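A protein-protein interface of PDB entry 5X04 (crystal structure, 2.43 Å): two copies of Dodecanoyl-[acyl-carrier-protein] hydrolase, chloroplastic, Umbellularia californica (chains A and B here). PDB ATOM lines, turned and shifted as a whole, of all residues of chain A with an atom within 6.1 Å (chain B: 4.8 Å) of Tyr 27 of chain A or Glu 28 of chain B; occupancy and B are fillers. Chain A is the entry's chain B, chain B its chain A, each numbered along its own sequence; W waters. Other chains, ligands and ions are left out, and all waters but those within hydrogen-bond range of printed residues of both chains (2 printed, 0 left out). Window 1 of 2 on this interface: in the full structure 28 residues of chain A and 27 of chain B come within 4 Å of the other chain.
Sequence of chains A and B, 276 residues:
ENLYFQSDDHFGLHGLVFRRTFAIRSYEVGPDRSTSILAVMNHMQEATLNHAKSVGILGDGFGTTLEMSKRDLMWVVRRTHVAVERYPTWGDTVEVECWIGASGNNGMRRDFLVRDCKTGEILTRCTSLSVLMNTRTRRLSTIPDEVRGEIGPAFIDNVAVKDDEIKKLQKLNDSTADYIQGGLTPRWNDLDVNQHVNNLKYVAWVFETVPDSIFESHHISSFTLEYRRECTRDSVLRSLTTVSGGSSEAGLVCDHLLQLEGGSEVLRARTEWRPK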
ATOM      1  N   ARG A  25      23.678 -17.173 -22.796  1.00  0.00           N
ATOM      2  CA  ARG A  25      23.340 -16.367 -23.952  1.00  0.00           C
ATOM      3  C   ARG A  25      24.409 -16.545 -25.013  1.00  0.00           C
ATOM      4  O   ARG A  25      25.523 -16.987 -24.725  1.00  0.00           O
ATOM      5  CB  ARG A  25      23.200 -14.891 -23.577  1.00  0.00           C
ATOM      6  CG  ARG A  25      22.040 -14.593 -22.643  1.00  0.00           C
ATOM      7  CD  ARG A  25      22.137 -13.180 -22.098  1.00  0.00           C
ATOM      8  NE  ARG A  25      21.123 -12.913 -21.082  1.00  0.00           N
ATOM      9  CZ  ARG A  25      20.940 -11.731 -20.505  1.00  0.00           C
ATOM     10  NH1 ARG A  25      21.703 -10.700 -20.844  1.00  0.00           N
ATOM     11  NH2 ARG A  25      19.992 -11.576 -19.591  1.00  0.00           N
ATOM     12  N   SER A  26      24.051 -16.204 -26.241  1.00  0.00           N
ATOM     13  CA  SER A  26      24.920 -16.399 -27.387  1.00  0.00           C
ATOM     14  C   SER A  26      26.240 -15.623 -27.287  1.00  0.00           C
ATOM     15  O   SER A  26      27.303 -16.172 -27.576  1.00  0.00           O
ATOM     16  CB  SER A  26      24.166 -16.033 -28.658  1.00  0.00           C
ATOM     17  OG  SER A  26      23.034 -16.868 -28.817  1.00  0.00           O
ATOM     18  N   TYR A  27      26.179 -14.354 -26.886  1.00  0.00           N
ATOM     19  CA  TYR A  27      27.385 -13.524 -26.839  1.00  0.00           C
ATOM     20  C   TYR A  27      28.281 -13.893 -25.658  1.00  0.00           C
ATOM     21  O   TYR A  27      29.377 -13.353 -25.508  1.00  0.00           O
ATOM     22  CB  TYR A  27      27.028 -12.037 -26.750  1.00  0.00           C
ATOM     23  CG  TYR A  27      26.279 -11.650 -25.490  1.00  0.00           C
ATOM     24  CD1 TYR A  27      26.967 -11.297 -24.331  1.00  0.00           C
ATOM     25  CD2 TYR A  27      24.893 -11.633 -25.456  1.00  0.00           C
ATOM     26  CE1 TYR A  27      26.294 -10.945 -23.179  1.00  0.00           C
ATOM     27  CE2 TYR A  27      24.211 -11.279 -24.306  1.00  0.00           C
ATOM     28  CZ  TYR A  27      24.917 -10.937 -23.172  1.00  0.00           C
ATOM     29  OH  TYR A  27      24.245 -10.584 -22.024  1.00  0.00           O
ATOM     30  N   GLU A  28      27.811 -14.816 -24.825  1.00  0.00           N
ATOM     31  CA  GLU A  28      28.562 -15.254 -23.654  1.00  0.00           C
ATOM     32  C   GLU A  28      29.397 -16.457 -24.037  1.00  0.00           C
ATOM     33  O   GLU A  28      30.225 -16.941 -23.266  1.00  0.00           O
ATOM     34  CB  GLU A  28      27.625 -15.616 -22.504  1.00  0.00           C
ATOM     35  CG  GLU A  28      26.946 -14.438 -21.843  1.00  0.00           C
ATOM     36  CD  GLU A  28      25.922 -14.877 -20.819  1.00  0.00           C
ATOM     37  OE1 GLU A  28      25.367 -15.985 -20.976  1.00  0.00           O
ATOM     38  OE2 GLU A  28      25.675 -14.121 -19.857  1.00  0.00           O
ATOM     39  N   VAL A  29      29.160 -16.928 -25.253  1.00  0.00           N
ATOM     40  CA  VAL A  29      29.787 -18.132 -25.756  1.00  0.00           C
ATOM     41  C   VAL A  29      30.795 -17.795 -26.854  1.00  0.00           C
ATOM     42  O   VAL A  29      30.533 -16.948 -27.709  1.00  0.00           O
ATOM     43  CB  VAL A  29      28.703 -19.103 -26.275  1.00  0.00           C
ATOM     44  CG1 VAL A  29      29.190 -19.894 -27.460  1.00  0.00           C
ATOM     45  CG2 VAL A  29      28.224 -20.015 -25.151  1.00  0.00           C
ATOM     46  N   GLY A  30      31.946 -18.460 -26.824  1.00  0.00           N
ATOM     47  CA  GLY A  30      32.993 -18.220 -27.800  1.00  0.00           C
ATOM     48  C   GLY A  30      32.787 -18.960 -29.107  1.00  0.00           C
ATOM     49  O   GLY A  30      31.814 -19.698 -29.259  1.00  0.00           O
ATOM     50  N   ALA B  23      15.559  -9.728 -17.100  1.00  0.00           N
ATOM     51  CA  ALA B  23      15.838  -8.902 -15.933  1.00  0.00           C
ATOM     52  C   ALA B  23      17.216  -8.268 -16.084  1.00  0.00           C
ATOM     53  O   ALA B  23      18.201  -8.972 -16.308  1.00  0.00           O
ATOM     54  CB  ALA B  23      15.758  -9.721 -14.659  1.00  0.00           C
ATOM     55  N   ILE B  24      17.285  -6.944 -15.973  1.00  0.00           N
ATOM     56  CA  ILE B  24      18.550  -6.237 -16.149  1.00  0.00           C
ATOM     57  C   ILE B  24      19.566  -6.669 -15.096  1.00  0.00           C
ATOM     58  O   ILE B  24      19.283  -6.651 -13.898  1.00  0.00           O
ATOM     59  CB  ILE B  24      18.362  -4.710 -16.078  1.00  0.00           C
ATOM     60  CG1 ILE B  24      17.385  -4.243 -17.158  1.00  0.00           C
ATOM     61  CG2 ILE B  24      19.696  -4.003 -16.244  1.00  0.00           C
ATOM     62  CD1 ILE B  24      17.766  -4.680 -18.558  1.00  0.00           C
ATOM     63  N   ARG B  25      20.753  -7.049 -15.556  1.00  0.00           N
ATOM     64  CA  ARG B  25      21.806  -7.529 -14.671  1.00  0.00           C
ATOM     65  C   ARG B  25      22.778  -6.408 -14.311  1.00  0.00           C
ATOM     66  O   ARG B  25      22.819  -5.373 -14.976  1.00  0.00           O
ATOM     67  CB  ARG B  25      22.549  -8.698 -15.321  1.00  0.00           C
ATOM     68  CG  ARG B  25      21.680  -9.934 -15.519  1.00  0.00           C
ATOM     69  CD  ARG B  25      22.353 -10.957 -16.419  1.00  0.00           C
ATOM     70  NE  ARG B  25      21.467 -12.073 -16.741  1.00  0.00           N
ATOM     71  CZ  ARG B  25      21.836 -13.140 -17.446  1.00  0.00           C
ATOM     72  NH1 ARG B  25      23.075 -13.238 -17.906  1.00  0.00           N
ATOM     73  NH2 ARG B  25      20.963 -14.108 -17.692  1.00  0.00           N
ATOM     74  N   SER B  26      23.552  -6.625 -13.251  1.00  0.00           N
ATOM     75  CA  SER B  26      24.451  -5.608 -12.708  1.00  0.00           C
ATOM     76  C   SER B  26      25.490  -5.110 -13.710  1.00  0.00           C
ATOM     77  O   SER B  26      25.710  -3.908 -13.840  1.00  0.00           O
ATOM     78  CB  SER B  26      25.162  -6.150 -11.468  1.00  0.00           C
ATOM     79  OG  SER B  26      25.875  -7.339 -11.763  1.00  0.00           O
ATOM     80  N   TYR B  27      26.132  -6.040 -14.408  1.00  0.00           N
ATOM     81  CA  TYR B  27      27.202  -5.695 -15.339  1.00  0.00           C
ATOM     82  C   TYR B  27      26.695  -5.062 -16.637  1.00  0.00           C
ATOM     83  O   TYR B  27      27.487  -4.698 -17.507  1.00  0.00           O
ATOM     84  CB  TYR B  27      28.049  -6.937 -15.643  1.00  0.00           C
ATOM     85  CG  TYR B  27      27.281  -8.100 -16.232  1.00  0.00           C
ATOM     86  CD1 TYR B  27      27.084  -8.214 -17.602  1.00  0.00           C
ATOM     87  CD2 TYR B  27      26.766  -9.097 -15.411  1.00  0.00           C
ATOM     88  CE1 TYR B  27      26.387  -9.283 -18.138  1.00  0.00           C
ATOM     89  CE2 TYR B  27      26.068 -10.168 -15.938  1.00  0.00           C
ATOM     90  CZ  TYR B  27      25.882 -10.256 -17.301  1.00  0.00           C
ATOM     91  OH  TYR B  27      25.189 -11.322 -17.828  1.00  0.00           O
ATOM     92  N   GLU B  28      25.378  -4.935 -16.765  1.00  0.00           N
ATOM     93  CA  GLU B  28      24.780  -4.349 -17.961  1.00  0.00           C
ATOM     94  C   GLU B  28      24.532  -2.847 -17.816  1.00  0.00           C
ATOM     95  O   GLU B  28      24.151  -2.182 -18.781  1.00  0.00           O
ATOM     96  CB  GLU B  28      23.472  -5.066 -18.302  1.00  0.00           C
ATOM     97  CG  GLU B  28      23.671  -6.469 -18.858  1.00  0.00           C
ATOM     98  CD  GLU B  28      22.366  -7.215 -19.054  1.00  0.00           C
ATOM     99  OE1 GLU B  28      21.397  -6.923 -18.322  1.00  0.00           O
ATOM    100  OE2 GLU B  28      22.309  -8.094 -19.939  1.00  0.00           O
ATOM    101  N   VAL B  29      24.743  -2.315 -16.616  1.00  0.00           N
ATOM    102  CA  VAL B  29      24.464  -0.904 -16.351  1.00  0.00           C
ATOM    103  C   VAL B  29      25.741  -0.091 -16.121  1.00  0.00           C
ATOM    104  O   VAL B  29      26.715  -0.578 -15.542  1.00  0.00           O
ATOM    105  CB  VAL B  29      23.517  -0.723 -15.140  1.00  0.00           C
ATOM    106  CG1 VAL B  29      22.272  -1.577 -15.309  1.00  0.00           C
ATOM    107  CG2 VAL B  29      24.220  -1.058 -13.833  1.00  0.00           C
ATOM    108  N   GLY B  30      25.738   1.142 -16.614  1.00  0.00           N
ATOM    109  CA  GLY B  30      26.876   2.028 -16.462  1.00  0.00           C
ATOM    110  C   GLY B  30      26.881   2.685 -15.095  1.00  0.00           C
ATOM    111  O   GLY B  30      25.989   2.433 -14.284  1.00  0.00           O
ATOM    112  N   SER B  34      22.265   3.374 -15.692  1.00  0.00           N
ATOM    113  CA  SER B  34      21.487   3.097 -16.893  1.00  0.00           C
ATOM    114  C   SER B  34      22.070   1.918 -17.657  1.00  0.00           C
ATOM    115  O   SER B  34      23.288   1.799 -17.794  1.00  0.00           O
ATOM    116  CB  SER B  34      21.431   4.326 -17.803  1.00  0.00           C
ATOM    117  OG  SER B  34      20.422   5.227 -17.388  1.00  0.00           O
ATOM    118  N   THR B  35      21.194   1.042 -18.141  1.00  0.00           N
ATOM    119  CA  THR B  35      21.599  -0.029 -19.041  1.00  0.00           C
ATOM    120  C   THR B  35      22.256   0.579 -20.273  1.00  0.00           C
ATOM    121  O   THR B  35      21.776   1.576 -20.808  1.00  0.00           O
ATOM    122  CB  THR B  35      20.396  -0.898 -19.464  1.00  0.00           C
ATOM    123  OG1 THR B  35      19.778  -1.462 -18.301  1.00  0.00           O
ATOM    124  CG2 THR B  35      20.834  -2.022 -20.388  1.00  0.00           C
ATOM    125  N   SER B  36      23.351  -0.019 -20.729  1.00  0.00           N
ATOM    126  CA  SER B  36      24.023   0.490 -21.915  1.00  0.00           C
ATOM    127  C   SER B  36      23.266   0.049 -23.155  1.00  0.00           C
ATOM    128  O   SER B  36      22.565  -0.961 -23.139  1.00  0.00           O
ATOM    129  CB  SER B  36      25.473   0.008 -21.970  1.00  0.00           C
ATOM    130  OG  SER B  36      25.538  -1.407 -22.028  1.00  0.00           O
ATOM    131  N   ALA B  39      24.010  -3.442 -24.172  1.00  0.00           N
ATOM    132  CA  ALA B  39      23.277  -4.493 -23.477  1.00  0.00           C
ATOM    133  C   ALA B  39      21.898  -4.667 -24.097  1.00  0.00           C
ATOM    134  O   ALA B  39      21.387  -5.778 -24.201  1.00  0.00           O
ATOM    135  CB  ALA B  39      23.167  -4.180 -21.995  1.00  0.00           C
ATOM    136  N   ASN B  42      22.413  -6.478 -27.302  1.00  0.00           N
ATOM    137  CA  ASN B  42      22.651  -7.875 -26.945  1.00  0.00           C
ATOM    138  C   ASN B  42      21.346  -8.627 -26.701  1.00  0.00           C
ATOM    139  O   ASN B  42      21.202  -9.783 -27.100  1.00  0.00           O
ATOM    140  CB  ASN B  42      23.548  -7.979 -25.710  1.00  0.00           C
ATOM    141  CG  ASN B  42      25.015  -7.759 -26.032  1.00  0.00           C
ATOM    142  OD1 ASN B  42      25.686  -8.650 -26.552  1.00  0.00           O
ATOM    143  ND2 ASN B  42      25.523  -6.579 -25.708  1.00  0.00           N
ATOM    144  N   HIS B  43      20.405  -7.965 -26.036  1.00  0.00           N
ATOM    145  CA  HIS B  43      19.102  -8.554 -25.741  1.00  0.00           C
ATOM    146  C   HIS B  43      18.356  -8.896 -27.021  1.00  0.00           C
ATOM    147  O   HIS B  43      17.781  -9.975 -27.153  1.00  0.00           O
ATOM    148  CB  HIS B  43      18.261  -7.597 -24.895  1.00  0.00           C
ATOM    149  CG  HIS B  43      18.850  -7.285 -23.558  1.00  0.00           C
ATOM    150  ND1 HIS B  43      18.481  -6.187 -22.816  1.00  0.00           N
ATOM    151  CD2 HIS B  43      19.782  -7.941 -22.816  1.00  0.00           C
ATOM    152  CE1 HIS B  43      19.159  -6.167 -21.683  1.00  0.00           C
ATOM    153  NE2 HIS B  43      19.955  -7.226 -21.662  1.00  0.00           N
HETATM  154  O   HOH W   1      23.538 -15.816 -19.402  1.00  0.00           O
HETATM  155  O   HOH W   2      19.385  -9.108 -18.761  1.00  0.00           O
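Of the printed residues of chain B, Tyr 27 of chain A touches Glu 28 (3.8 Å) and Asn 42 (3.2 Å).
Of the printed residues of chain B, Glu 28 of chain A touches Arg 25 and Tyr 27.
Of the printed residues of chain A, Tyr 27 of chain B touches Glu 28.
Of the printed residues of chain B, Arg 25 of chain A touches Arg 25 (3.2 Å), Glu 28 (2.8 Å) and His 43 (3.9 Å).
The nearest residue of chain B that does not touch Tyr 27 of chain A is Tyr 27 of chain B (4.4 Å).
The nearest printed residue of chain A that does not touch Glu 28 of chain B is Glu 28 of chain A (6.9 Å).
The nearest printed residue of chain A that does not touch His 43 of chain B is Tyr 27 of chain A (5.2 Å).
The guanidinium group of Arg 25 of chain B is in salt-bridge range of the side-chain carboxylate of Glu 28 of chain A (3.4 Å).
The side-chain carboxylate (OE2) of Glu 28 of chain A sits at hydrogen-bond distance from the side-chain hydroxyl (OH) of Tyr 27 of chain B (3.5 Å).
The side-chain carboxylate (OE2) of Glu 28 of chain B is in salt-bridge range of the guanidinium group (NH1) of Arg 25 of chain A.
The guanidinium group (NE) of Arg 25 of chain B sits close to the guanidinium group (NH2) of Arg 25 of chain A (3.2 Å).
Arg 25 of chain A touches its own counterpart, Arg 25 of chain B.
Arg 25 of chain A touches Glu 28 of chain B, and with the chains exchanged Glu 28 of chain A touches Arg 25 of chain B.
Tyr 27 of chain A touches Glu 28 of chain B, and with the chains exchanged Glu 28 of chain A touches Tyr 27 of chain B.
Of the 7 pairs that touch across the chains among the printed residues, 5 have their exchanged pair printed and touching as well.
Of the 6 printed residues of chain A, 3 touch a printed residue of chain B.
Printed residues of chain B that touch a printed residue of chain A: Arg 25, Tyr 27, Glu 28, Asn 42 and His 43.
Hydrophobic or aromatic side chains of chain B that line the printed part of chain A: Tyr 27 and His 43.
Among the printed residues, 7 pairs touch across the chains.
Among the printed residues, Asp or Glu carboxylates within 4 Å of a Lys or Arg side-chain nitrogen of the other chain: Arg 25 of chain A with Glu 28 of chain B and Glu 28 of chain A with Arg 25 of chain B.
Water W1 bridges OE1 of Glu 28 of chain A (2.4 Å) and NH1 of Arg 25 of chain B (3.0 Å).
Water W2 lies within hydrogen-bond range of the guanidinium group (NH2) of Arg 25 of chain A (2.7 Å), the backbone carbonyl oxygen (O) of Ala 23 of chain B (2.7 Å) and the side-chain carboxylate (OE1) of Glu 28 of chain B (3.0 Å).
The backbone NH (N) of Arg 25 of chain A lies within hydrogen-bond range of the side-chain carboxylate (OE1) of Glu 28 of chain A.
The side-chain carboxylate of Glu 28 of chain B sits at hydrogen-bond distance from the backbone NH of Arg 25 of chain B.
The backbone NH (N) of Ser 36 of chain B sits at hydrogen-bond distance from the backbone carbonyl oxygen (O) of Glu 28 of chain B.
The side-chain hydroxyl (OH) of Tyr 27 of chain A lies within hydrogen-bond range of the guanidinium group (NH1) of Arg 25 of chain A, at 2.8 Å.
The backbone carbonyl oxygen of Ala 39 of chain B lies close to a ring nitrogen (ND1) of His 43 of chain B (3.2 Å).
The guanidinium group (NH1) of Arg 25 of chain B lies within hydrogen-bond range of the side-chain hydroxyl (OH) of Tyr 27 of chain B.
His 43 of chain B touches Arg 25 of chain A.
OH of Tyr 27 of chain A touches OE2 of Glu 28 of chain B, at 3.8 Å.
Tyr 27 of chain A touches Asn 42 of chain B (CG to OD1, 3.2 Å).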
